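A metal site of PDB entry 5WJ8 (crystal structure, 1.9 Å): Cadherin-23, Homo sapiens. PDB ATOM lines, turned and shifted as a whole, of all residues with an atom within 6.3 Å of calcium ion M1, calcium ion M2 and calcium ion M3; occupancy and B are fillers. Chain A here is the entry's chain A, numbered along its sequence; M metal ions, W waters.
Calcium ion M2 is bound by the side-chain carboxylate of Glu 74 (2.2 Å), water W1 (2.3 Å), water W2 (2.3 Å), the side-chain carboxylate of Asp 72 (2.3 Å), the side-chain carboxylate of Glu 18 (2.4 Å) and the side-chain carboxylate of Asp 107 (2.4 Å). Calcium ion M2 has six donor atoms within binding distance.
Within 4 Å of calcium ion M1: Glu 18, Glu 74, Asp 104, Glu 105, Asp 107 and Asp 141.
Calcium ion M1 is bound by OE1 of Glu 18 (2.3 Å). OD1 of Asp 107 binds calcium ion M1, 2.3 Å away. Calcium ion M1 is bound by OD1 of Asp 141, at 2.3 Å. OD1 of Asp 104 is bound to calcium ion M1 (2.4 Å). O of Glu 105 is bound to calcium ion M1, 2.4 Å away. Calcium ion M1 is bound by the side-chain carboxylate (OE2) of Glu 74, at 2.5 Å. OE1 of Glu 74 binds calcium ion M1. Calcium ion M1 has seven donor atoms within binding distance.
Calcium ion M3 is bound by the backbone carbonyl oxygen (O) of Asn 108 (2.3 Å), the backbone carbonyl oxygen (O) of Asn 145 (2.3 Å), the side-chain amide oxygen (OD1) of Asn 106 (2.4 Å), the side-chain carboxylate (OD2) of Asp 141 (2.4 Å), the side-chain carboxylate (OD2) of Asp 139 (2.4 Å), the side-chain carboxylate (OD2) of Asp 195 (2.5 Å) and the side-chain carboxylate (OD1) of Asp 139 (2.7 Å). Calcium ion M3 has seven donor atoms within binding distance.
OE2 of Glu 74 sits close to NH2 of Arg 73 (2.9 Å). The backbone NH (N) of Glu 18 is in hydrogen-bond range of the backbone carbonyl oxygen (O) of Leu 103 (3.1 Å). ND2 of Asn 108 sits close to OD1 of Asp 107 (3.0 Å). The side-chain carboxylate (OD2) of Asp 104 lies within hydrogen-bond range of the side-chain amide nitrogen (ND2) of Asn 145. The side-chain carboxylate (OD2) of Asp 104 sits at hydrogen-bond distance from the backbone NH (N) of Ala 142, at 3.0 Å. The side-chain amide nitrogen (ND2) of Asn 19 lies within hydrogen-bond range of the side-chain carboxylate (OE1) of Glu 105 (3.1 Å). The backbone carbonyl oxygen of Arg 201 is in hydrogen-bond range of the backbone NH of Asp 195 (2.9 Å). The backbone NH (N) of Gly 197 sits at hydrogen-bond distance from the side-chain carboxylate (OD1) of Asp 195, 2.9 Å away.
Four residues have an atom within 4 Å of calcium ion M2: Glu 18, Asp 72, Glu 74 and Asp 107. Along chain A the residues within 4 Å of calcium ion M2 span positions 18 to 107. The nearest printed residue that does not touch calcium ion M2 is Arg 73 (4.2 Å).
Of the 27 residues printed, 6 come within 4 Å of calcium ion M3. The nearest printed residue that does not touch calcium ion M3 is Gly 146 (4.4 Å).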
ATOM      1  N   GLU A  18     -11.184 -11.825  33.676  1.00  0.00           N
ATOM      2  CA  GLU A  18     -12.038 -12.773  32.941  1.00  0.00           C
ATOM      3  C   GLU A  18     -11.494 -14.200  33.087  1.00  0.00           C
ATOM      4  O   GLU A  18     -10.328 -14.390  33.429  1.00  0.00           O
ATOM      5  CB  GLU A  18     -12.149 -12.407  31.462  1.00  0.00           C
ATOM      6  CG  GLU A  18     -10.836 -12.310  30.691  1.00  0.00           C
ATOM      7  CD  GLU A  18     -11.062 -12.192  29.185  1.00  0.00           C
ATOM      8  OE1 GLU A  18     -10.179 -11.673  28.471  1.00  0.00           O
ATOM      9  OE2 GLU A  18     -12.130 -12.646  28.709  1.00  0.00           O
ATOM     10  N   ASN A  19     -12.347 -15.179  32.810  1.00  0.00           N
ATOM     11  CA  ASN A  19     -12.015 -16.620  32.802  1.00  0.00           C
ATOM     12  C   ASN A  19     -11.781 -17.250  34.196  1.00  0.00           C
ATOM     13  O   ASN A  19     -11.322 -18.375  34.305  1.00  0.00           O
ATOM     14  CB  ASN A  19     -10.827 -16.946  31.872  1.00  0.00           C
ATOM     15  CG  ASN A  19     -11.058 -16.518  30.425  1.00  0.00           C
ATOM     16  OD1 ASN A  19     -12.166 -16.659  29.879  1.00  0.00           O
ATOM     17  ND2 ASN A  19     -10.019 -15.997  29.787  1.00  0.00           N
ATOM     18  N   VAL A  71     -17.164 -16.018  32.591  1.00  0.00           N
ATOM     19  CA  VAL A  71     -16.972 -14.581  32.514  1.00  0.00           C
ATOM     20  C   VAL A  71     -15.987 -14.258  31.383  1.00  0.00           C
ATOM     21  O   VAL A  71     -14.795 -14.651  31.459  1.00  0.00           O
ATOM     22  CB  VAL A  71     -16.467 -13.988  33.849  1.00  0.00           C
ATOM     23  CG1 VAL A  71     -16.171 -12.501  33.731  1.00  0.00           C
ATOM     24  CG2 VAL A  71     -17.504 -14.200  34.934  1.00  0.00           C
ATOM     25  N   ASP A  72     -16.500 -13.588  30.334  1.00  0.00           N
ATOM     26  CA  ASP A  72     -15.734 -13.333  29.112  1.00  0.00           C
ATOM     27  C   ASP A  72     -15.734 -11.845  28.852  1.00  0.00           C
ATOM     28  O   ASP A  72     -16.779 -11.275  28.526  1.00  0.00           O
ATOM     29  CB  ASP A  72     -16.348 -14.113  27.956  1.00  0.00           C
ATOM     30  CG  ASP A  72     -15.609 -13.939  26.636  1.00  0.00           C
ATOM     31  OD1 ASP A  72     -14.576 -13.239  26.567  1.00  0.00           O
ATOM     32  OD2 ASP A  72     -16.099 -14.493  25.645  1.00  0.00           O
ATOM     33  N   ARG A  73     -14.576 -11.198  28.993  1.00  0.00           N
ATOM     34  CA  ARG A  73     -14.479  -9.763  28.769  1.00  0.00           C
ATOM     35  C   ARG A  73     -14.891  -9.394  27.335  1.00  0.00           C
ATOM     36  O   ARG A  73     -15.459  -8.328  27.098  1.00  0.00           O
ATOM     37  CB  ARG A  73     -13.062  -9.235  29.034  1.00  0.00           C
ATOM     38  CG  ARG A  73     -13.021  -7.709  29.189  1.00  0.00           C
ATOM     39  CD  ARG A  73     -11.749  -7.120  28.639  1.00  0.00           C
ATOM     40  NE  ARG A  73     -11.625  -7.436  27.214  1.00  0.00           N
ATOM     41  CZ  ARG A  73     -12.136  -6.723  26.205  1.00  0.00           C
ATOM     42  NH1 ARG A  73     -12.779  -5.568  26.411  1.00  0.00           N
ATOM     43  NH2 ARG A  73     -11.966  -7.162  24.965  1.00  0.00           N
ATOM     44  N   GLU A  74     -14.635 -10.297  26.396  1.00  0.00           N
ATOM     45  CA  GLU A  74     -15.019 -10.074  25.000  1.00  0.00           C
ATOM     46  C   GLU A  74     -16.556 -10.011  24.791  1.00  0.00           C
ATOM     47  O   GLU A  74     -17.019  -9.476  23.780  1.00  0.00           O
ATOM     48  CB  GLU A  74     -14.391 -11.141  24.104  1.00  0.00           C
ATOM     49  CG  GLU A  74     -12.928 -10.894  23.771  1.00  0.00           C
ATOM     50  CD  GLU A  74     -11.980 -10.955  24.974  1.00  0.00           C
ATOM     51  OE1 GLU A  74     -11.882 -12.003  25.662  1.00  0.00           O
ATOM     52  OE2 GLU A  74     -11.308  -9.949  25.238  1.00  0.00           O
ATOM     53  N   LYS A  75     -17.340 -10.549  25.725  1.00  0.00           N
ATOM     54  CA  LYS A  75     -18.815 -10.462  25.671  1.00  0.00           C
ATOM     55  C   LYS A  75     -19.412  -9.383  26.572  1.00  0.00           C
ATOM     56  O   LYS A  75     -20.568  -9.052  26.426  1.00  0.00           O
ATOM     57  CB  LYS A  75     -19.421 -11.822  26.046  1.00  0.00           C
ATOM     58  CG  LYS A  75     -19.222 -12.886  24.986  1.00  0.00           C
ATOM     59  CD  LYS A  75     -19.910 -14.190  25.374  1.00  0.00           C
ATOM     60  CE  LYS A  75     -19.665 -15.343  24.399  1.00  0.00           C
ATOM     61  NZ  LYS A  75     -19.257 -14.958  23.016  1.00  0.00           N
ATOM     62  N   LEU A 103     -11.660  -7.389  33.729  1.00  0.00           N
ATOM     63  CA  LEU A 103     -10.377  -7.001  33.169  1.00  0.00           C
ATOM     64  C   LEU A 103      -9.943  -8.017  32.128  1.00  0.00           C
ATOM     65  O   LEU A 103     -10.291  -9.206  32.235  1.00  0.00           O
ATOM     66  CB  LEU A 103      -9.306  -6.996  34.279  1.00  0.00           C
ATOM     67  CG  LEU A 103      -9.583  -6.174  35.544  1.00  0.00           C
ATOM     68  CD1 LEU A 103      -8.441  -6.293  36.550  1.00  0.00           C
ATOM     69  CD2 LEU A 103      -9.786  -4.704  35.190  1.00  0.00           C
ATOM     70  N   ASP A 104      -9.128  -7.554  31.188  1.00  0.00           N
ATOM     71  CA  ASP A 104      -8.716  -8.351  30.041  1.00  0.00           C
ATOM     72  C   ASP A 104      -7.586  -9.324  30.345  1.00  0.00           C
ATOM     73  O   ASP A 104      -6.626  -8.956  31.023  1.00  0.00           O
ATOM     74  CB  ASP A 104      -8.249  -7.436  28.902  1.00  0.00           C
ATOM     75  CG  ASP A 104      -8.187  -8.154  27.563  1.00  0.00           C
ATOM     76  OD1 ASP A 104      -9.087  -8.938  27.207  1.00  0.00           O
ATOM     77  OD2 ASP A 104      -7.229  -7.924  26.823  1.00  0.00           O
ATOM     78  N   GLU A 105      -7.729 -10.539  29.832  1.00  0.00           N
ATOM     79  CA  GLU A 105      -6.642 -11.499  29.652  1.00  0.00           C
ATOM     80  C   GLU A 105      -6.343 -11.629  28.187  1.00  0.00           C
ATOM     81  O   GLU A 105      -7.245 -11.497  27.328  1.00  0.00           O
ATOM     82  CB  GLU A 105      -7.021 -12.874  30.186  1.00  0.00           C
ATOM     83  CG  GLU A 105      -6.952 -12.883  31.710  1.00  0.00           C
ATOM     84  CD  GLU A 105      -7.125 -14.257  32.319  1.00  0.00           C
ATOM     85  OE1 GLU A 105      -7.682 -15.167  31.639  1.00  0.00           O
ATOM     86  OE2 GLU A 105      -6.709 -14.388  33.495  1.00  0.00           O
ATOM     87  N   ASN A 106      -5.086 -11.945  27.892  1.00  0.00           N
ATOM     88  CA  ASN A 106      -4.670 -12.183  26.519  1.00  0.00           C
ATOM     89  C   ASN A 106      -5.046 -13.613  26.126  1.00  0.00           C
ATOM     90  O   ASN A 106      -4.190 -14.478  25.915  1.00  0.00           O
ATOM     91  CB  ASN A 106      -3.182 -11.906  26.322  1.00  0.00           C
ATOM     92  CG  ASN A 106      -2.847 -11.734  24.858  1.00  0.00           C
ATOM     93  OD1 ASN A 106      -3.744 -11.455  24.075  1.00  0.00           O
ATOM     94  ND2 ASN A 106      -1.579 -11.911  24.467  1.00  0.00           N
ATOM     95  N   ASP A 107      -6.344 -13.846  25.977  1.00  0.00           N
ATOM     96  CA  ASP A 107      -6.858 -15.187  25.814  1.00  0.00           C
ATOM     97  C   ASP A 107      -7.219 -15.492  24.360  1.00  0.00           C
ATOM     98  O   ASP A 107      -7.815 -16.513  24.080  1.00  0.00           O
ATOM     99  CB  ASP A 107      -7.995 -15.500  26.804  1.00  0.00           C
ATOM    100  CG  ASP A 107      -9.220 -14.580  26.676  1.00  0.00           C
ATOM    101  OD1 ASP A 107      -9.171 -13.459  26.126  1.00  0.00           O
ATOM    102  OD2 ASP A 107     -10.255 -14.983  27.218  1.00  0.00           O
ATOM    103  N   ASN A 108      -6.802 -14.613  23.450  1.00  0.00           N
ATOM    104  CA  ASN A 108      -6.947 -14.858  22.023  1.00  0.00           C
ATOM    105  C   ASN A 108      -5.648 -14.592  21.294  1.00  0.00           C
ATOM    106  O   ASN A 108      -4.954 -13.604  21.567  1.00  0.00           O
ATOM    107  CB  ASN A 108      -8.065 -13.982  21.424  1.00  0.00           C
ATOM    108  CG  ASN A 108      -9.416 -14.285  22.024  1.00  0.00           C
ATOM    109  OD1 ASN A 108     -10.158 -15.127  21.507  1.00  0.00           O
ATOM    110  ND2 ASN A 108      -9.727 -13.644  23.138  1.00  0.00           N
ATOM    111  N   SER A 109      -5.335 -15.484  20.357  1.00  0.00           N
ATOM    112  CA  SER A 109      -4.289 -15.275  19.369  1.00  0.00           C
ATOM    113  C   SER A 109      -4.911 -14.616  18.140  1.00  0.00           C
ATOM    114  O   SER A 109      -6.095 -14.798  17.881  1.00  0.00           O
ATOM    115  CB  SER A 109      -3.696 -16.609  18.910  1.00  0.00           C
ATOM    116  OG  SER A 109      -3.100 -17.301  19.988  1.00  0.00           O
ATOM    117  N   PRO A 110      -4.100 -13.877  17.359  1.00  0.00           N
ATOM    118  CA  PRO A 110      -4.571 -13.407  16.055  1.00  0.00           C
ATOM    119  C   PRO A 110      -5.079 -14.563  15.215  1.00  0.00           C
ATOM    120  O   PRO A 110      -4.490 -15.633  15.225  1.00  0.00           O
ATOM    121  CB  PRO A 110      -3.302 -12.807  15.435  1.00  0.00           C
ATOM    122  CG  PRO A 110      -2.500 -12.336  16.604  1.00  0.00           C
ATOM    123  CD  PRO A 110      -2.770 -13.338  17.696  1.00  0.00           C
ATOM    124  N   ASP A 139      -7.899  -9.818  16.282  1.00  0.00           N
ATOM    125  CA  ASP A 139      -7.663 -10.214  17.659  1.00  0.00           C
ATOM    126  C   ASP A 139      -8.615  -9.385  18.526  1.00  0.00           C
ATOM    127  O   ASP A 139      -8.423  -8.182  18.645  1.00  0.00           O
ATOM    128  CB  ASP A 139      -6.216  -9.981  18.020  1.00  0.00           C
ATOM    129  CG  ASP A 139      -5.827 -10.610  19.349  1.00  0.00           C
ATOM    130  OD1 ASP A 139      -6.601 -10.508  20.332  1.00  0.00           O
ATOM    131  OD2 ASP A 139      -4.719 -11.197  19.407  1.00  0.00           O
ATOM    132  N   PRO A 140      -9.611 -10.043  19.159  1.00  0.00           N
ATOM    133  CA  PRO A 140     -10.643  -9.357  19.933  1.00  0.00           C
ATOM    134  C   PRO A 140     -10.266  -8.876  21.347  1.00  0.00           C
ATOM    135  O   PRO A 140     -11.111  -8.282  22.017  1.00  0.00           O
ATOM    136  CB  PRO A 140     -11.738 -10.421  20.038  1.00  0.00           C
ATOM    137  CG  PRO A 140     -10.978 -11.707  20.059  1.00  0.00           C
ATOM    138  CD  PRO A 140      -9.861 -11.497  19.110  1.00  0.00           C
ATOM    139  N   ASP A 141      -9.039  -9.113  21.812  1.00  0.00           N
ATOM    140  CA  ASP A 141      -8.641  -8.656  23.147  1.00  0.00           C
ATOM    141  C   ASP A 141      -8.517  -7.120  23.194  1.00  0.00           C
ATOM    142  O   ASP A 141      -8.489  -6.455  22.163  1.00  0.00           O
ATOM    143  CB  ASP A 141      -7.323  -9.318  23.587  1.00  0.00           C
ATOM    144  CG  ASP A 141      -7.444 -10.840  23.729  1.00  0.00           C
ATOM    145  OD1 ASP A 141      -8.421 -11.357  24.310  1.00  0.00           O
ATOM    146  OD2 ASP A 141      -6.516 -11.542  23.255  1.00  0.00           O
ATOM    147  N   ALA A 142      -8.415  -6.566  24.397  1.00  0.00           N
ATOM    148  CA  ALA A 142      -8.328  -5.140  24.603  1.00  0.00           C
ATOM    149  C   ALA A 142      -6.905  -4.621  24.555  1.00  0.00           C
ATOM    150  O   ALA A 142      -5.959  -5.369  24.810  1.00  0.00           O
ATOM    151  CB  ALA A 142      -8.991  -4.743  25.912  1.00  0.00           C
ATOM    152  N   SER A 144      -3.247  -3.351  24.008  1.00  0.00           N
ATOM    153  CA  SER A 144      -2.107  -4.084  23.431  1.00  0.00           C
ATOM    154  C   SER A 144      -2.379  -5.555  23.113  1.00  0.00           C
ATOM    155  O   SER A 144      -1.898  -6.066  22.087  1.00  0.00           O
ATOM    156  CB  SER A 144      -0.909  -4.014  24.371  1.00  0.00           C
ATOM    157  OG  SER A 144      -0.437  -2.686  24.456  1.00  0.00           O
ATOM    158  N   ASN A 145      -3.134  -6.243  23.960  1.00  0.00           N
ATOM    159  CA  ASN A 145      -3.456  -7.665  23.771  1.00  0.00           C
ATOM    160  C   ASN A 145      -4.166  -7.962  22.452  1.00  0.00           C
ATOM    161  O   ASN A 145      -4.105  -9.122  21.984  1.00  0.00           O
ATOM    162  CB  ASN A 145      -4.336  -8.217  24.906  1.00  0.00           C
ATOM    163  CG  ASN A 145      -3.596  -8.369  26.226  1.00  0.00           C
ATOM    164  OD1 ASN A 145      -2.373  -8.439  26.268  1.00  0.00           O
ATOM    165  ND2 ASN A 145      -4.371  -8.468  27.305  1.00  0.00           N
ATOM    166  N   GLY A 146      -4.866  -6.971  21.925  1.00  0.00           N
ATOM    167  CA  GLY A 146      -5.633  -7.096  20.692  1.00  0.00           C
ATOM    168  C   GLY A 146      -5.077  -6.355  19.492  1.00  0.00           C
ATOM    169  O   GLY A 146      -5.669  -6.389  18.425  1.00  0.00           O
ATOM    170  N   GLN A 147      -3.950  -5.671  19.650  1.00  0.00           N
ATOM    171  CA  GLN A 147      -3.242  -5.033  18.527  1.00  0.00           C
ATOM    172  C   GLN A 147      -2.395  -6.036  17.776  1.00  0.00           C
ATOM    173  O   GLN A 147      -1.615  -6.727  18.402  1.00  0.00           O
ATOM    174  CB  GLN A 147      -2.323  -3.930  19.048  1.00  0.00           C
ATOM    175  CG  GLN A 147      -3.118  -2.742  19.541  1.00  0.00           C
ATOM    176  CD  GLN A 147      -2.264  -1.655  20.145  1.00  0.00           C
ATOM    177  OE1 GLN A 147      -1.154  -1.895  20.639  1.00  0.00           O
ATOM    178  NE2 GLN A 147      -2.796  -0.449  20.138  1.00  0.00           N
ATOM    179  N   ASP A 195       0.162 -10.515  18.352  1.00  0.00           N
ATOM    180  CA  ASP A 195      -0.424  -9.436  19.147  1.00  0.00           C
ATOM    181  C   ASP A 195       0.698  -8.737  19.923  1.00  0.00           C
ATOM    182  O   ASP A 195       1.866  -9.122  19.814  1.00  0.00           O
ATOM    183  CB  ASP A 195      -1.607  -9.866  20.024  1.00  0.00           C
ATOM    184  CG  ASP A 195      -1.240 -10.829  21.140  1.00  0.00           C
ATOM    185  OD1 ASP A 195      -0.092 -10.780  21.655  1.00  0.00           O
ATOM    186  OD2 ASP A 195      -2.122 -11.648  21.510  1.00  0.00           O
ATOM    187  N   ARG A 196       0.371  -7.706  20.694  1.00  0.00           N
ATOM    188  CA  ARG A 196       1.338  -7.047  21.546  1.00  0.00           C
ATOM    189  C   ARG A 196       1.101  -7.320  23.023  1.00  0.00           C
ATOM    190  O   ARG A 196       1.363  -6.472  23.848  1.00  0.00           O
ATOM    191  CB  ARG A 196       1.323  -5.549  21.323  1.00  0.00           C
ATOM    192  CG  ARG A 196       1.599  -5.123  19.907  1.00  0.00           C
ATOM    193  CD  ARG A 196       1.626  -3.606  19.850  1.00  0.00           C
ATOM    194  NE  ARG A 196       2.678  -3.149  18.959  1.00  0.00           N
ATOM    195  CZ  ARG A 196       2.517  -2.695  17.709  1.00  0.00           C
ATOM    196  NH1 ARG A 196       1.302  -2.602  17.143  1.00  0.00           N
ATOM    197  NH2 ARG A 196       3.590  -2.345  17.019  1.00  0.00           N
ATOM    198  N   GLY A 197       0.625  -8.515  23.356  1.00  0.00           N
ATOM    199  CA  GLY A 197       0.602  -8.959  24.748  1.00  0.00           C
ATOM    200  C   GLY A 197       2.017  -9.202  25.264  1.00  0.00           C
ATOM    201  O   GLY A 197       2.975  -9.188  24.498  1.00  0.00           O
ATOM    202  N   ARG A 201       1.219 -13.387  21.616  1.00  0.00           N
ATOM    203  CA  ARG A 201       0.649 -14.584  21.024  1.00  0.00           C
ATOM    204  C   ARG A 201       0.729 -14.389  19.531  1.00  0.00           C
ATOM    205  O   ARG A 201       0.572 -13.264  19.032  1.00  0.00           O
ATOM    206  CB  ARG A 201      -0.795 -14.761  21.453  1.00  0.00           C
ATOM    207  CG  ARG A 201      -0.903 -14.974  22.956  1.00  0.00           C
ATOM    208  CD  ARG A 201      -2.302 -15.230  23.468  1.00  0.00           C
ATOM    209  NE  ARG A 201      -2.947 -16.394  22.849  1.00  0.00           N
ATOM    210  CZ  ARG A 201      -3.844 -17.173  23.426  1.00  0.00           C
ATOM    211  NH1 ARG A 201      -4.290 -16.953  24.667  1.00  0.00           N
ATOM    212  NH2 ARG A 201      -4.321 -18.210  22.740  1.00  0.00           N
HETATM  213 CA    CA M   1      -9.467 -11.147  26.401  1.00  0.00          CA
HETATM  214 CA    CA M   2     -12.325 -13.869  26.652  1.00  0.00          CA
HETATM  215 CA    CA M   3      -4.589 -11.378  21.831  1.00  0.00          CA
HETATM  216  O   HOH W   1     -12.141 -14.833  24.555  1.00  0.00           O
HETATM  217  O   HOH W   2     -13.247 -15.731  27.695  1.00  0.00           O
